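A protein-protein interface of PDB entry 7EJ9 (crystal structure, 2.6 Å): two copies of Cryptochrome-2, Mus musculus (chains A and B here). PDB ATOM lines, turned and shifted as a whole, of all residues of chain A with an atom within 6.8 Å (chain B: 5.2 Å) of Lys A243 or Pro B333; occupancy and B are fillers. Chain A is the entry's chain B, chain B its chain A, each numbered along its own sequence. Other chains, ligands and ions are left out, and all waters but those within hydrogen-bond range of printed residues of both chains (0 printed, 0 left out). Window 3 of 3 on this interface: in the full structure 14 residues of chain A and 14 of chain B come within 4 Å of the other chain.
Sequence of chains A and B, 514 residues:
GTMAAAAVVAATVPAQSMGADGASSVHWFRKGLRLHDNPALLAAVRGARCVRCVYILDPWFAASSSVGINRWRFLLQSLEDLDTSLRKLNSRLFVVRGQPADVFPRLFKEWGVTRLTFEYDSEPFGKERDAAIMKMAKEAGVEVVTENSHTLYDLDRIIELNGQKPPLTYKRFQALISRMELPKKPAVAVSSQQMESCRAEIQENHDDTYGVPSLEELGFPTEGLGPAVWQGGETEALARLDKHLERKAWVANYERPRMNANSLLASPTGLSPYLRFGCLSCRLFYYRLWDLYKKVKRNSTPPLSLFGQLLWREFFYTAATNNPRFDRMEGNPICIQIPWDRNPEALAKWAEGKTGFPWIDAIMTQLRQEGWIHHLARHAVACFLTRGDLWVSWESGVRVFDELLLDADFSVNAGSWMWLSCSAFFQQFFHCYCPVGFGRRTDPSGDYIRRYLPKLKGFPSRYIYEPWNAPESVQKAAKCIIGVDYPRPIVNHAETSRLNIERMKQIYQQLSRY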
ATOM      1  N   LEU A 238     -26.555   5.241 -17.149  1.00  0.00           N
ATOM      2  CA  LEU A 238     -26.259   4.685 -18.465  1.00  0.00           C
ATOM      3  C   LEU A 238     -25.213   3.583 -18.367  1.00  0.00           C
ATOM      4  O   LEU A 238     -25.293   2.573 -19.082  1.00  0.00           O
ATOM      5  CB  LEU A 238     -25.797   5.796 -19.404  1.00  0.00           C
ATOM      6  CG  LEU A 238     -26.911   6.769 -19.796  1.00  0.00           C
ATOM      7  CD1 LEU A 238     -26.361   7.949 -20.573  1.00  0.00           C
ATOM      8  CD2 LEU A 238     -27.988   6.045 -20.600  1.00  0.00           C
ATOM      9  N   ALA A 239     -24.233   3.751 -17.471  1.00  0.00           N
ATOM     10  CA  ALA A 239     -23.234   2.710 -17.271  1.00  0.00           C
ATOM     11  C   ALA A 239     -23.865   1.455 -16.686  1.00  0.00           C
ATOM     12  O   ALA A 239     -23.557   0.342 -17.120  1.00  0.00           O
ATOM     13  CB  ALA A 239     -22.110   3.220 -16.373  1.00  0.00           C
ATOM     14  N   ARG A 240     -24.757   1.614 -15.706  1.00  0.00           N
ATOM     15  CA  ARG A 240     -25.432   0.455 -15.135  1.00  0.00           C
ATOM     16  C   ARG A 240     -26.324  -0.227 -16.164  1.00  0.00           C
ATOM     17  O   ARG A 240     -26.393  -1.461 -16.215  1.00  0.00           O
ATOM     18  CB  ARG A 240     -26.248   0.867 -13.909  1.00  0.00           C
ATOM     19  CG  ARG A 240     -25.422   1.038 -12.646  1.00  0.00           C
ATOM     20  CD  ARG A 240     -26.233   1.684 -11.542  1.00  0.00           C
ATOM     21  NE  ARG A 240     -25.559   1.606 -10.252  1.00  0.00           N
ATOM     22  CZ  ARG A 240     -25.801   0.673  -9.342  1.00  0.00           C
ATOM     23  NH1 ARG A 240     -26.714  -0.263  -9.540  1.00  0.00           N
ATOM     24  NH2 ARG A 240     -25.109   0.676  -8.210  1.00  0.00           N
ATOM     25  N   LEU A 241     -27.003   0.560 -17.003  1.00  0.00           N
ATOM     26  CA  LEU A 241     -27.906  -0.015 -17.998  1.00  0.00           C
ATOM     27  C   LEU A 241     -27.160  -0.951 -18.940  1.00  0.00           C
ATOM     28  O   LEU A 241     -27.620  -2.064 -19.219  1.00  0.00           O
ATOM     29  CB  LEU A 241     -28.602   1.099 -18.779  1.00  0.00           C
ATOM     30  CG  LEU A 241     -29.424   0.696 -20.005  1.00  0.00           C
ATOM     31  CD1 LEU A 241     -30.737   0.048 -19.605  1.00  0.00           C
ATOM     32  CD2 LEU A 241     -29.663   1.903 -20.883  1.00  0.00           C
ATOM     33  N   ASP A 242     -25.995  -0.521 -19.432  1.00  0.00           N
ATOM     34  CA  ASP A 242     -25.189  -1.384 -20.293  1.00  0.00           C
ATOM     35  C   ASP A 242     -24.759  -2.646 -19.557  1.00  0.00           C
ATOM     36  O   ASP A 242     -24.855  -3.753 -20.095  1.00  0.00           O
ATOM     37  CB  ASP A 242     -23.969  -0.625 -20.814  1.00  0.00           C
ATOM     38  CG  ASP A 242     -24.330   0.422 -21.848  1.00  0.00           C
ATOM     39  OD1 ASP A 242     -25.516   0.503 -22.221  1.00  0.00           O
ATOM     40  OD2 ASP A 242     -23.432   1.170 -22.288  1.00  0.00           O
ATOM     41  N   LYS A 243     -24.280  -2.503 -18.318  1.00  0.00           N
ATOM     42  CA  LYS A 243     -23.867  -3.669 -17.542  1.00  0.00           C
ATOM     43  C   LYS A 243     -25.043  -4.554 -17.166  1.00  0.00           C
ATOM     44  O   LYS A 243     -24.851  -5.751 -16.928  1.00  0.00           O
ATOM     45  CB  LYS A 243     -23.125  -3.230 -16.286  1.00  0.00           C
ATOM     46  CG  LYS A 243     -21.909  -2.386 -16.580  1.00  0.00           C
ATOM     47  CD  LYS A 243     -20.882  -3.165 -17.369  1.00  0.00           C
ATOM     48  CE  LYS A 243     -20.213  -2.264 -18.375  1.00  0.00           C
ATOM     49  NZ  LYS A 243     -18.974  -2.882 -18.888  1.00  0.00           N
ATOM     50  N   HIS A 244     -26.250  -3.990 -17.108  1.00  0.00           N
ATOM     51  CA  HIS A 244     -27.440  -4.775 -16.808  1.00  0.00           C
ATOM     52  C   HIS A 244     -27.858  -5.614 -18.007  1.00  0.00           C
ATOM     53  O   HIS A 244     -28.254  -6.773 -17.849  1.00  0.00           O
ATOM     54  CB  HIS A 244     -28.574  -3.847 -16.380  1.00  0.00           C
ATOM     55  CG  HIS A 244     -29.863  -4.547 -16.083  1.00  0.00           C
ATOM     56  ND1 HIS A 244     -30.253  -4.877 -14.802  1.00  0.00           N
ATOM     57  CD2 HIS A 244     -30.860  -4.959 -16.899  1.00  0.00           C
ATOM     58  CE1 HIS A 244     -31.432  -5.469 -14.843  1.00  0.00           C
ATOM     59  NE2 HIS A 244     -31.822  -5.532 -16.103  1.00  0.00           N
ATOM     60  N   LEU A 245     -27.773  -5.042 -19.210  1.00  0.00           N
ATOM     61  CA  LEU A 245     -28.127  -5.789 -20.411  1.00  0.00           C
ATOM     62  C   LEU A 245     -27.070  -6.828 -20.756  1.00  0.00           C
ATOM     63  O   LEU A 245     -27.404  -7.896 -21.287  1.00  0.00           O
ATOM     64  CB  LEU A 245     -28.334  -4.825 -21.578  1.00  0.00           C
ATOM     65  CG  LEU A 245     -29.359  -3.713 -21.317  1.00  0.00           C
ATOM     66  CD1 LEU A 245     -29.341  -2.690 -22.440  1.00  0.00           C
ATOM     67  CD2 LEU A 245     -30.767  -4.272 -21.107  1.00  0.00           C
ATOM     68  N   GLU A 246     -25.800  -6.539 -20.462  1.00  0.00           N
ATOM     69  CA  GLU A 246     -24.736  -7.508 -20.705  1.00  0.00           C
ATOM     70  C   GLU A 246     -24.889  -8.735 -19.816  1.00  0.00           C
ATOM     71  O   GLU A 246     -24.659  -9.865 -20.265  1.00  0.00           O
ATOM     72  CB  GLU A 246     -23.374  -6.850 -20.492  1.00  0.00           C
ATOM     73  CG  GLU A 246     -23.065  -5.769 -21.511  1.00  0.00           C
ATOM     74  CD  GLU A 246     -22.039  -4.757 -21.025  1.00  0.00           C
ATOM     75  OE1 GLU A 246     -21.331  -5.028 -20.025  1.00  0.00           O
ATOM     76  OE2 GLU A 246     -21.943  -3.682 -21.657  1.00  0.00           O
ATOM     77  N   ARG A 247     -25.278  -8.534 -18.553  1.00  0.00           N
ATOM     78  CA  ARG A 247     -25.513  -9.663 -17.656  1.00  0.00           C
ATOM     79  C   ARG A 247     -26.683 -10.511 -18.142  1.00  0.00           C
ATOM     80  O   ARG A 247     -26.573 -11.740 -18.244  1.00  0.00           O
ATOM     81  CB  ARG A 247     -25.764  -9.163 -16.232  1.00  0.00           C
ATOM     82  N   LYS A 248     -27.811  -9.866 -18.460  1.00  0.00           N
ATOM     83  CA  LYS A 248     -28.981 -10.598 -18.936  1.00  0.00           C
ATOM     84  C   LYS A 248     -28.645 -11.445 -20.159  1.00  0.00           C
ATOM     85  O   LYS A 248     -29.110 -12.585 -20.282  1.00  0.00           O
ATOM     86  CB  LYS A 248     -30.114  -9.616 -19.242  1.00  0.00           C
ATOM     87  CG  LYS A 248     -31.510 -10.232 -19.253  1.00  0.00           C
ATOM     88  CD  LYS A 248     -32.559  -9.207 -18.821  1.00  0.00           C
ATOM     89  CE  LYS A 248     -33.973  -9.732 -19.035  1.00  0.00           C
ATOM     90  NZ  LYS A 248     -35.009  -8.753 -18.570  1.00  0.00           N
ATOM     91  N   PRO A 268     -24.960  -3.986  -8.223  1.00  0.00           N
ATOM     92  CA  PRO A 268     -24.248  -2.942  -8.974  1.00  0.00           C
ATOM     93  C   PRO A 268     -24.757  -2.749 -10.391  1.00  0.00           C
ATOM     94  O   PRO A 268     -24.230  -1.887 -11.103  1.00  0.00           O
ATOM     95  CB  PRO A 268     -22.799  -3.442  -8.979  1.00  0.00           C
ATOM     96  CG  PRO A 268     -22.919  -4.918  -8.813  1.00  0.00           C
ATOM     97  CD  PRO A 268     -24.086  -5.127  -7.899  1.00  0.00           C
ATOM     98  N   THR A 269     -25.745  -3.523 -10.839  1.00  0.00           N
ATOM     99  CA  THR A 269     -26.414  -3.262 -12.106  1.00  0.00           C
ATOM    100  C   THR A 269     -27.880  -2.907 -11.905  1.00  0.00           C
ATOM    101  O   THR A 269     -28.631  -2.815 -12.886  1.00  0.00           O
ATOM    102  CB  THR A 269     -26.288  -4.461 -13.051  1.00  0.00           C
ATOM    103  OG1 THR A 269     -27.121  -5.524 -12.583  1.00  0.00           O
ATOM    104  CG2 THR A 269     -24.844  -4.943 -13.113  1.00  0.00           C
ATOM    105  N   ARG A 288     -34.046  -0.988 -25.315  1.00  0.00           N
ATOM    106  CA  ARG A 288     -32.806  -1.753 -25.211  1.00  0.00           C
ATOM    107  C   ARG A 288     -33.084  -3.160 -24.697  1.00  0.00           C
ATOM    108  O   ARG A 288     -32.460  -4.130 -25.146  1.00  0.00           O
ATOM    109  CB  ARG A 288     -31.812  -1.032 -24.298  1.00  0.00           C
ATOM    110  CG  ARG A 288     -31.237   0.248 -24.887  1.00  0.00           C
ATOM    111  CD  ARG A 288     -30.083  -0.047 -25.824  1.00  0.00           C
ATOM    112  NE  ARG A 288     -28.969  -0.643 -25.100  1.00  0.00           N
ATOM    113  CZ  ARG A 288     -28.071   0.052 -24.417  1.00  0.00           C
ATOM    114  NH1 ARG A 288     -28.108   1.374 -24.374  1.00  0.00           N
ATOM    115  NH2 ARG A 288     -27.112  -0.594 -23.766  1.00  0.00           N
ATOM    116  N   LYS B 165     -17.729  -3.784 -24.463  1.00  0.00           N
ATOM    117  CA  LYS B 165     -17.672  -4.265 -23.095  1.00  0.00           C
ATOM    118  C   LYS B 165     -16.420  -5.126 -22.946  1.00  0.00           C
ATOM    119  O   LYS B 165     -15.952  -5.702 -23.934  1.00  0.00           O
ATOM    120  CB  LYS B 165     -18.917  -5.087 -22.728  1.00  0.00           C
ATOM    121  N   PRO B 166     -15.841  -5.222 -21.753  1.00  0.00           N
ATOM    122  CA  PRO B 166     -14.669  -6.086 -21.577  1.00  0.00           C
ATOM    123  C   PRO B 166     -15.086  -7.543 -21.493  1.00  0.00           C
ATOM    124  O   PRO B 166     -16.149  -7.860 -20.941  1.00  0.00           O
ATOM    125  CB  PRO B 166     -14.071  -5.596 -20.252  1.00  0.00           C
ATOM    126  CG  PRO B 166     -15.263  -5.146 -19.480  1.00  0.00           C
ATOM    127  CD  PRO B 166     -16.236  -4.567 -20.492  1.00  0.00           C
ATOM    128  N   ASN B 323     -13.201   0.048 -15.419  1.00  0.00           N
ATOM    129  CA  ASN B 323     -13.970  -0.235 -14.208  1.00  0.00           C
ATOM    130  C   ASN B 323     -13.206   0.320 -13.011  1.00  0.00           C
ATOM    131  O   ASN B 323     -12.404  -0.396 -12.394  1.00  0.00           O
ATOM    132  CB  ASN B 323     -14.211  -1.736 -14.065  1.00  0.00           C
ATOM    133  CG  ASN B 323     -15.008  -2.091 -12.823  1.00  0.00           C
ATOM    134  OD1 ASN B 323     -15.386  -1.222 -12.033  1.00  0.00           O
ATOM    135  ND2 ASN B 323     -15.283  -3.378 -12.655  1.00  0.00           N
ATOM    136  N   GLY B 331     -21.038  -1.735  -5.911  1.00  0.00           N
ATOM    137  CA  GLY B 331     -20.995  -0.868  -7.066  1.00  0.00           C
ATOM    138  C   GLY B 331     -20.195  -1.399  -8.228  1.00  0.00           C
ATOM    139  O   GLY B 331     -20.182  -0.761  -9.289  1.00  0.00           O
ATOM    140  N   ASN B 332     -19.540  -2.552  -8.067  1.00  0.00           N
ATOM    141  CA  ASN B 332     -18.680  -3.114  -9.100  1.00  0.00           C
ATOM    142  C   ASN B 332     -19.511  -4.024  -9.990  1.00  0.00           C
ATOM    143  O   ASN B 332     -19.898  -5.118  -9.552  1.00  0.00           O
ATOM    144  CB  ASN B 332     -17.536  -3.886  -8.456  1.00  0.00           C
ATOM    145  CG  ASN B 332     -16.580  -4.476  -9.465  1.00  0.00           C
ATOM    146  OD1 ASN B 332     -16.657  -4.190 -10.660  1.00  0.00           O
ATOM    147  ND2 ASN B 332     -15.668  -5.310  -8.989  1.00  0.00           N
ATOM    148  N   PRO B 333     -19.787  -3.643 -11.246  1.00  0.00           N
ATOM    149  CA  PRO B 333     -20.770  -4.388 -12.056  1.00  0.00           C
ATOM    150  C   PRO B 333     -20.432  -5.854 -12.263  1.00  0.00           C
ATOM    151  O   PRO B 333     -21.341  -6.675 -12.453  1.00  0.00           O
ATOM    152  CB  PRO B 333     -20.759  -3.642 -13.399  1.00  0.00           C
ATOM    153  CG  PRO B 333     -20.093  -2.368 -13.153  1.00  0.00           C
ATOM    154  CD  PRO B 333     -19.152  -2.560 -12.010  1.00  0.00           C
ATOM    155  N   ILE B 334     -19.144  -6.207 -12.246  1.00  0.00           N
ATOM    156  CA  ILE B 334     -18.732  -7.576 -12.520  1.00  0.00           C
ATOM    157  C   ILE B 334     -18.689  -8.443 -11.275  1.00  0.00           C
ATOM    158  O   ILE B 334     -18.509  -9.665 -11.393  1.00  0.00           O
ATOM    159  CB  ILE B 334     -17.342  -7.593 -13.179  1.00  0.00           C
ATOM    160  CG1 ILE B 334     -16.296  -7.103 -12.177  1.00  0.00           C
ATOM    161  CG2 ILE B 334     -17.350  -6.717 -14.410  1.00  0.00           C
ATOM    162  CD1 ILE B 334     -14.908  -7.625 -12.434  1.00  0.00           C
ATOM    163  N   CYS B 335     -18.848  -7.862 -10.088  1.00  0.00           N
ATOM    164  CA  CYS B 335     -18.592  -8.565  -8.838  1.00  0.00           C
ATOM    165  C   CYS B 335     -19.885  -9.063  -8.209  1.00  0.00           C
ATOM    166  O   CYS B 335     -20.884  -8.342  -8.153  1.00  0.00           O
ATOM    167  CB  CYS B 335     -17.845  -7.662  -7.851  1.00  0.00           C
ATOM    168  SG  CYS B 335     -17.353  -8.524  -6.338  1.00  0.00           S
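A ring nitrogen (ND1) of His A244 is in hydrogen-bond range of the backbone carbonyl oxygen (O) of Thr A269 (3.2 Å). The side-chain amide nitrogen (ND2) of Asn B323 sits at hydrogen-bond distance from the side-chain amide oxygen (OD1) of Asn B332. The guanidinium group (NH1) of Arg A240 lies close to the backbone carbonyl oxygen (O) of Pro A268 (3.4 Å). OE1 of Glu A246 lies within salt-bridge range of NZ of Lys A243 (3.4 Å).
Among the printed residues, pairs that only touch across the chains: Lys A243 with Pro B166 (3.6 Å), Lys A243 with Pro B333 (3.6 Å), Glu A246 with Lys B165 (3.5 Å), Pro A268 with Gly B331 (3.4 Å), Pro A268 with Asn B332 (3.1 Å), Pro A268 with Pro B333 (3.8 Å) and Thr A269 with Pro B333 (3.96 Å).
Lys A243 touches two residues of chain B. Pro B333 touches just these residues of chain A: Lys A243, Pro A268 and Thr A269. Of the printed residues of chain A, Asn B332 touches Pro A268. Of the printed residues of chain A, Gly B331 touches Pro A268. Printed residues of chain B within 4 Å of Glu A246: Lys B165. Of the printed residues of chain B, Thr A269 touches Pro B333 (3.96 Å). His A244 touches none of the printed residues of chain B. Arg A288 touches none of the printed residues of chain B. The nearest printed residue of chain B that does not touch Glu A246 is Pro B166 (5.1 Å).
No position is printed for both chains.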
